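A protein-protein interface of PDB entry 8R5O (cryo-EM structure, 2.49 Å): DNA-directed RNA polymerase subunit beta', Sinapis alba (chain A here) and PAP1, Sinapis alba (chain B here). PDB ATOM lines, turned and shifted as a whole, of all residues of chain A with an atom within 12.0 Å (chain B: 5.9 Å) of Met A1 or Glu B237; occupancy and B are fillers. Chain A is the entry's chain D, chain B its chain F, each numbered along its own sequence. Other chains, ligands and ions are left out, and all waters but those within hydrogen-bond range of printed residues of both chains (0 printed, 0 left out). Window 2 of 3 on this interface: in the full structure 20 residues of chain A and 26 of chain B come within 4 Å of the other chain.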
ATOM      1  N   MET A   1      -3.615  11.914  23.160  1.00  0.00           N
ATOM      2  CA  MET A   1      -3.523  13.112  22.335  1.00  0.00           C
ATOM      3  C   MET A   1      -2.124  13.284  21.752  1.00  0.00           C
ATOM      4  O   MET A   1      -1.187  12.593  22.146  1.00  0.00           O
ATOM      5  CB  MET A   1      -3.912  14.352  23.147  1.00  0.00           C
ATOM      6  CG  MET A   1      -3.447  14.333  24.599  1.00  0.00           C
ATOM      7  SD  MET A   1      -1.668  14.551  24.825  1.00  0.00           S
ATOM      8  CE  MET A   1      -1.480  16.288  24.428  1.00  0.00           C
ATOM      9  N   ILE A   2      -1.994  14.208  20.809  1.00  0.00           N
ATOM     10  CA  ILE A   2      -0.702  14.553  20.230  1.00  0.00           C
ATOM     11  C   ILE A   2      -0.045  15.604  21.112  1.00  0.00           C
ATOM     12  O   ILE A   2      -0.637  16.653  21.387  1.00  0.00           O
ATOM     13  CB  ILE A   2      -0.862  15.069  18.790  1.00  0.00           C
ATOM     14  CG1 ILE A   2      -1.661  14.074  17.951  1.00  0.00           C
ATOM     15  CG2 ILE A   2       0.499  15.312  18.158  1.00  0.00           C
ATOM     16  CD1 ILE A   2      -2.015  14.589  16.578  1.00  0.00           C
ATOM     17  N   ASP A   3       1.179  15.324  21.553  1.00  0.00           N
ATOM     18  CA  ASP A   3       1.915  16.285  22.361  1.00  0.00           C
ATOM     19  C   ASP A   3       2.146  17.572  21.580  1.00  0.00           C
ATOM     20  O   ASP A   3       2.332  17.562  20.360  1.00  0.00           O
ATOM     21  CB  ASP A   3       3.259  15.705  22.797  1.00  0.00           C
ATOM     22  CG  ASP A   3       3.119  14.394  23.532  1.00  0.00           C
ATOM     23  OD1 ASP A   3       2.042  14.147  24.112  1.00  0.00           O
ATOM     24  OD2 ASP A   3       4.087  13.608  23.530  1.00  0.00           O
ATOM     25  N   ARG A   4       2.123  18.692  22.294  1.00  0.00           N
ATOM     26  CA  ARG A   4       2.505  19.974  21.711  1.00  0.00           C
ATOM     27  C   ARG A   4       4.024  19.995  21.638  1.00  0.00           C
ATOM     28  O   ARG A   4       4.700  20.340  22.609  1.00  0.00           O
ATOM     29  CB  ARG A   4       1.964  21.135  22.538  1.00  0.00           C
ATOM     30  CG  ARG A   4       0.523  20.970  22.991  1.00  0.00           C
ATOM     31  CD  ARG A   4      -0.430  20.763  21.823  1.00  0.00           C
ATOM     32  NE  ARG A   4      -0.463  21.905  20.920  1.00  0.00           N
ATOM     33  CZ  ARG A   4      -1.435  22.140  20.048  1.00  0.00           C
ATOM     34  NH1 ARG A   4      -2.485  21.342  19.955  1.00  0.00           N
ATOM     35  NH2 ARG A   4      -1.354  23.206  19.257  1.00  0.00           N
ATOM     36  N   TYR A   5       4.567  19.612  20.487  1.00  0.00           N
ATOM     37  CA  TYR A   5       6.006  19.436  20.358  1.00  0.00           C
ATOM     38  C   TYR A   5       6.730  20.772  20.451  1.00  0.00           C
ATOM     39  O   TYR A   5       6.276  21.786  19.916  1.00  0.00           O
ATOM     40  CB  TYR A   5       6.343  18.748  19.038  1.00  0.00           C
ATOM     41  CG  TYR A   5       5.651  17.421  18.848  1.00  0.00           C
ATOM     42  CD1 TYR A   5       5.919  16.348  19.688  1.00  0.00           C
ATOM     43  CD2 TYR A   5       4.736  17.235  17.824  1.00  0.00           C
ATOM     44  CE1 TYR A   5       5.289  15.134  19.517  1.00  0.00           C
ATOM     45  CE2 TYR A   5       4.102  16.021  17.643  1.00  0.00           C
ATOM     46  CZ  TYR A   5       4.382  14.976  18.493  1.00  0.00           C
ATOM     47  OH  TYR A   5       3.753  13.765  18.320  1.00  0.00           O
ATOM     48  N   LYS A   6       7.869  20.763  21.136  1.00  0.00           N
ATOM     49  CA  LYS A   6       8.690  21.955  21.314  1.00  0.00           C
ATOM     50  C   LYS A   6      10.145  21.525  21.234  1.00  0.00           C
ATOM     51  O   LYS A   6      10.651  20.869  22.150  1.00  0.00           O
ATOM     52  CB  LYS A   6       8.390  22.640  22.647  1.00  0.00           C
ATOM     53  CG  LYS A   6       9.231  23.870  22.916  1.00  0.00           C
ATOM     54  CD  LYS A   6       8.800  24.560  24.196  1.00  0.00           C
ATOM     55  CE  LYS A   6       9.647  25.790  24.472  1.00  0.00           C
ATOM     56  NZ  LYS A   6       9.151  26.550  25.652  1.00  0.00           N
ATOM     57  N   ILE B 232      -3.913  20.104  10.864  1.00  0.00           N
ATOM     58  CA  ILE B 232      -5.174  19.376  10.761  1.00  0.00           C
ATOM     59  C   ILE B 232      -5.303  18.362  11.891  1.00  0.00           C
ATOM     60  O   ILE B 232      -6.355  18.255  12.532  1.00  0.00           O
ATOM     61  CB  ILE B 232      -5.289  18.705   9.381  1.00  0.00           C
ATOM     62  CG1 ILE B 232      -5.336  19.765   8.283  1.00  0.00           C
ATOM     63  CG2 ILE B 232      -6.516  17.812   9.319  1.00  0.00           C
ATOM     64  CD1 ILE B 232      -5.304  19.195   6.893  1.00  0.00           C
ATOM     65  N   SER B 233      -4.235  17.606  12.157  1.00  0.00           N
ATOM     66  CA  SER B 233      -4.294  16.592  13.205  1.00  0.00           C
ATOM     67  C   SER B 233      -4.525  17.212  14.577  1.00  0.00           C
ATOM     68  O   SER B 233      -5.155  16.589  15.439  1.00  0.00           O
ATOM     69  CB  SER B 233      -3.014  15.757  13.199  1.00  0.00           C
ATOM     70  OG  SER B 233      -1.864  16.577  13.287  1.00  0.00           O
ATOM     71  N   TYR B 234      -4.026  18.429  14.801  1.00  0.00           N
ATOM     72  CA  TYR B 234      -4.350  19.143  16.031  1.00  0.00           C
ATOM     73  C   TYR B 234      -5.829  19.504  16.086  1.00  0.00           C
ATOM     74  O   TYR B 234      -6.461  19.401  17.144  1.00  0.00           O
ATOM     75  CB  TYR B 234      -3.489  20.398  16.155  1.00  0.00           C
ATOM     76  CG  TYR B 234      -2.101  20.147  16.695  1.00  0.00           C
ATOM     77  CD1 TYR B 234      -1.863  19.129  17.607  1.00  0.00           C
ATOM     78  CD2 TYR B 234      -1.028  20.930  16.294  1.00  0.00           C
ATOM     79  CE1 TYR B 234      -0.593  18.898  18.104  1.00  0.00           C
ATOM     80  CE2 TYR B 234       0.241  20.706  16.784  1.00  0.00           C
ATOM     81  CZ  TYR B 234       0.455  19.690  17.688  1.00  0.00           C
ATOM     82  OH  TYR B 234       1.721  19.470  18.177  1.00  0.00           O
ATOM     83  N   GLU B 235      -6.397  19.939  14.958  1.00  0.00           N
ATOM     84  CA  GLU B 235      -7.822  20.246  14.918  1.00  0.00           C
ATOM     85  C   GLU B 235      -8.668  18.982  15.000  1.00  0.00           C
ATOM     86  O   GLU B 235      -9.779  19.016  15.542  1.00  0.00           O
ATOM     87  CB  GLU B 235      -8.161  21.029  13.650  1.00  0.00           C
ATOM     88  CG  GLU B 235      -7.447  22.365  13.523  1.00  0.00           C
ATOM     89  CD  GLU B 235      -7.892  23.376  14.564  1.00  0.00           C
ATOM     90  OE1 GLU B 235      -8.984  23.203  15.142  1.00  0.00           O
ATOM     91  OE2 GLU B 235      -7.145  24.348  14.802  1.00  0.00           O
ATOM     92  N   MET B 236      -8.167  17.869  14.465  1.00  0.00           N
ATOM     93  CA  MET B 236      -8.904  16.612  14.531  1.00  0.00           C
ATOM     94  C   MET B 236      -9.116  16.170  15.973  1.00  0.00           C
ATOM     95  O   MET B 236     -10.204  15.711  16.336  1.00  0.00           O
ATOM     96  CB  MET B 236      -8.163  15.535  13.737  1.00  0.00           C
ATOM     97  CG  MET B 236      -8.860  14.192  13.699  1.00  0.00           C
ATOM     98  SD  MET B 236      -7.935  12.958  12.769  1.00  0.00           S
ATOM     99  CE  MET B 236      -6.465  12.806  13.775  1.00  0.00           C
ATOM    100  N   GLU B 237      -8.088  16.305  16.812  1.00  0.00           N
ATOM    101  CA  GLU B 237      -8.221  15.935  18.216  1.00  0.00           C
ATOM    102  C   GLU B 237      -9.034  16.961  18.995  1.00  0.00           C
ATOM    103  O   GLU B 237      -9.742  16.603  19.943  1.00  0.00           O
ATOM    104  CB  GLU B 237      -6.841  15.756  18.846  1.00  0.00           C
ATOM    105  CG  GLU B 237      -6.074  14.565  18.310  1.00  0.00           C
ATOM    106  CD  GLU B 237      -4.876  14.219  19.164  1.00  0.00           C
ATOM    107  OE1 GLU B 237      -4.344  15.124  19.842  1.00  0.00           O
ATOM    108  OE2 GLU B 237      -4.469  13.038  19.165  1.00  0.00           O
ATOM    109  N   ALA B 238      -8.939  18.238  18.620  1.00  0.00           N
ATOM    110  CA  ALA B 238      -9.750  19.261  19.272  1.00  0.00           C
ATOM    111  C   ALA B 238     -11.234  19.011  19.041  1.00  0.00           C
ATOM    112  O   ALA B 238     -12.058  19.245  19.933  1.00  0.00           O
ATOM    113  CB  ALA B 238      -9.354  20.649  18.768  1.00  0.00           C
ATOM    114  N   ALA B 239     -11.594  18.538  17.847  1.00  0.00           N
ATOM    115  CA  ALA B 239     -12.980  18.174  17.579  1.00  0.00           C
ATOM    116  C   ALA B 239     -13.424  17.014  18.463  1.00  0.00           C
ATOM    117  O   ALA B 239     -14.560  16.995  18.948  1.00  0.00           O
ATOM    118  CB  ALA B 239     -13.156  17.824  16.103  1.00  0.00           C
ATOM    119  N   GLY B 240     -12.543  16.042  18.685  1.00  0.00           N
ATOM    120  CA  GLY B 240     -12.860  14.912  19.535  1.00  0.00           C
ATOM    121  C   GLY B 240     -12.476  13.572  18.942  1.00  0.00           C
ATOM    122  O   GLY B 240     -12.849  12.523  19.475  1.00  0.00           O
ATOM    123  N   ARG B 241     -11.733  13.593  17.840  1.00  0.00           N
ATOM    124  CA  ARG B 241     -11.264  12.384  17.168  1.00  0.00           C
ATOM    125  C   ARG B 241      -9.767  12.260  17.429  1.00  0.00           C
ATOM    126  O   ARG B 241      -8.970  13.027  16.881  1.00  0.00           O
ATOM    127  CB  ARG B 241     -11.574  12.442  15.673  1.00  0.00           C
ATOM    128  CG  ARG B 241     -11.534  11.101  14.945  1.00  0.00           C
ATOM    129  CD  ARG B 241     -10.128  10.734  14.507  1.00  0.00           C
ATOM    130  NE  ARG B 241     -10.092   9.518  13.703  1.00  0.00           N
ATOM    131  CZ  ARG B 241     -10.110   9.496  12.378  1.00  0.00           C
ATOM    132  NH1 ARG B 241     -10.180  10.611  11.670  1.00  0.00           N
ATOM    133  NH2 ARG B 241     -10.054   8.327  11.748  1.00  0.00           N
ATOM    134  N   PHE B 242      -9.388  11.293  18.260  1.00  0.00           N
ATOM    135  CA  PHE B 242      -7.994  11.128  18.645  1.00  0.00           C
ATOM    136  C   PHE B 242      -7.191  10.487  17.520  1.00  0.00           C
ATOM    137  O   PHE B 242      -7.677   9.596  16.818  1.00  0.00           O
ATOM    138  CB  PHE B 242      -7.890  10.278  19.911  1.00  0.00           C
ATOM    139  CG  PHE B 242      -8.638  10.844  21.080  1.00  0.00           C
ATOM    140  CD1 PHE B 242      -8.645  12.208  21.320  1.00  0.00           C
ATOM    141  CD2 PHE B 242      -9.346  10.016  21.934  1.00  0.00           C
ATOM    142  CE1 PHE B 242      -9.337  12.733  22.393  1.00  0.00           C
ATOM    143  CE2 PHE B 242     -10.040  10.535  23.009  1.00  0.00           C
ATOM    144  CZ  PHE B 242     -10.034  11.896  23.239  1.00  0.00           C
ATOM    145  N   ALA B 243      -5.956  10.952  17.356  1.00  0.00           N
ATOM    146  CA  ALA B 243      -5.073  10.397  16.340  1.00  0.00           C
ATOM    147  C   ALA B 243      -4.674   8.970  16.693  1.00  0.00           C
ATOM    148  O   ALA B 243      -4.507   8.626  17.866  1.00  0.00           O
ATOM    149  CB  ALA B 243      -3.829  11.268  16.185  1.00  0.00           C
ATOM    150  N   PHE B 248      -0.072   9.105  12.921  1.00  0.00           N
ATOM    151  CA  PHE B 248       1.304   9.345  13.338  1.00  0.00           C
ATOM    152  C   PHE B 248       2.294   8.856  12.289  1.00  0.00           C
ATOM    153  O   PHE B 248       3.316   9.505  12.042  1.00  0.00           O
ATOM    154  CB  PHE B 248       1.573   8.671  14.683  1.00  0.00           C
ATOM    155  CG  PHE B 248       1.022   9.421  15.861  1.00  0.00           C
ATOM    156  CD1 PHE B 248       1.586  10.621  16.257  1.00  0.00           C
ATOM    157  CD2 PHE B 248      -0.046   8.919  16.582  1.00  0.00           C
ATOM    158  CE1 PHE B 248       1.088  11.311  17.341  1.00  0.00           C
ATOM    159  CE2 PHE B 248      -0.550   9.604  17.668  1.00  0.00           C
ATOM    160  CZ  PHE B 248       0.017  10.801  18.049  1.00  0.00           C
ATOM    161  N   ASN B 270       5.620   9.899  21.943  1.00  0.00           N
ATOM    162  CA  ASN B 270       4.185  10.134  22.064  1.00  0.00           C
ATOM    163  C   ASN B 270       3.402   8.845  21.839  1.00  0.00           C
ATOM    164  O   ASN B 270       2.380   8.608  22.491  1.00  0.00           O
ATOM    165  CB  ASN B 270       3.755  11.211  21.065  1.00  0.00           C
ATOM    166  CG  ASN B 270       2.431  11.860  21.425  1.00  0.00           C
ATOM    167  OD1 ASN B 270       2.140  12.969  20.981  1.00  0.00           O
ATOM    168  ND2 ASN B 270       1.628  11.182  22.234  1.00  0.00           N
ATOM    169  N   MET B 278      -2.610   4.145  19.759  1.00  0.00           N
ATOM    170  CA  MET B 278      -1.479   4.944  19.311  1.00  0.00           C
ATOM    171  C   MET B 278      -0.168   4.172  19.297  1.00  0.00           C
ATOM    172  O   MET B 278       0.866   4.753  18.965  1.00  0.00           O
ATOM    173  CB  MET B 278      -1.323   6.178  20.204  1.00  0.00           C
ATOM    174  CG  MET B 278      -2.513   7.109  20.197  1.00  0.00           C
ATOM    175  SD  MET B 278      -2.616   8.103  21.697  1.00  0.00           S
ATOM    176  CE  MET B 278      -1.015   8.897  21.693  1.00  0.00           C
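The backbone carbonyl oxygen (O) of Asp A3 lies within hydrogen-bond range of the side-chain hydroxyl (OH) of Tyr B234 (3.0 Å). OD1 of Asn B270 sits at hydrogen-bond distance from N of Asp A3 (2.6 Å). OD1 of Asn B270 is in hydrogen-bond range of OH of Tyr A5 (3.2 Å). The side-chain carboxylate (OE1) of Glu B237 sits at hydrogen-bond distance from the backbone NH (N) of Ile A2 (2.7 Å). The backbone carbonyl oxygen of Met A1 is in hydrogen-bond range of the side-chain amide nitrogen of Asn B270, at 3.2 Å.
The side-chain carboxylate (OE2) of Glu B237 is in hydrogen-bond range of the backbone NH (N) of Ala B243.
Among the printed residues, merely in contact across the chains: Arg A4 with Tyr B234, Met A1 with Glu B237, Ile A2 with Asn B270, Tyr A5 with Tyr B234, Ile A2 with Phe B248, Ile A2 with Ser B233, Met A1 with Met B278, Ile A2 with Tyr B234, Tyr A5 with Phe B248 and Ile A2 with Ala B243.
Of chain A, only Met A1 (3.3 Å) and Ile A2 (2.7 Å) come within 4 Å of Glu B237. Ser B233 touches just one residue of chain A: Ile A2 (3.7 Å). Printed residues of chain A within 4 Å of Tyr B234: Ile A2 (3.7 Å), Asp A3 (3.0 Å), Arg A4 (3.3 Å) and Tyr A5 (3.7 Å). Met B236 touches none of the printed residues of chain A. No residue of chain A comes within 4 Å of Ala B239. No residue of chain A comes within 4 Å of Gly B240. Ala B243 touches just one residue of chain A: Ile A2. Of chain A, only Met A1 (3.2 Å), Ile A2 (3.3 Å), Asp A3 (2.6 Å) and Tyr A5 (3.2 Å) come within 4 Å of Asn B270. Printed residues of chain B within 4 Å of Ile A2: Ser B233, Tyr B234, Glu B237, Ala B243, Phe B248 and Asn B270. Of the printed residues of chain B, Asp A3 touches Tyr B234 and Asn B270. Of the printed residues of chain A, Phe B248 touches Ile A2 and Tyr A5. Printed residues of chain A within 4 Å of Met B278: Met A1 (3.7 Å). Glu B235 touches none of the printed residues of chain A. The nearest residue of chain A that does not touch Glu B237 is Asp A3 (5.8 Å). The nearest printed residue of chain A that does not touch Met B278 is Ile A2 (5.5 Å).
Of the 15 printed residues of chain B, 7 touch a printed residue of chain A. Printed residues of chain B that touch a printed residue of chain A: Ser B233, Tyr B234, Glu B237, Ala B243, Phe B248, Asn B270 and Met B278. Hydrophobic or aromatic side chains of chain B that line the printed part of chain A: Tyr B234, Ala B243, Phe B248 and Met B278. Of the 6 printed residues of chain A, 5 touch a printed residue of chain B. Among the printed residues, no Asp or Glu carboxylate lies within 4 Å of a Lys or Arg side-chain nitrogen of the other chain.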
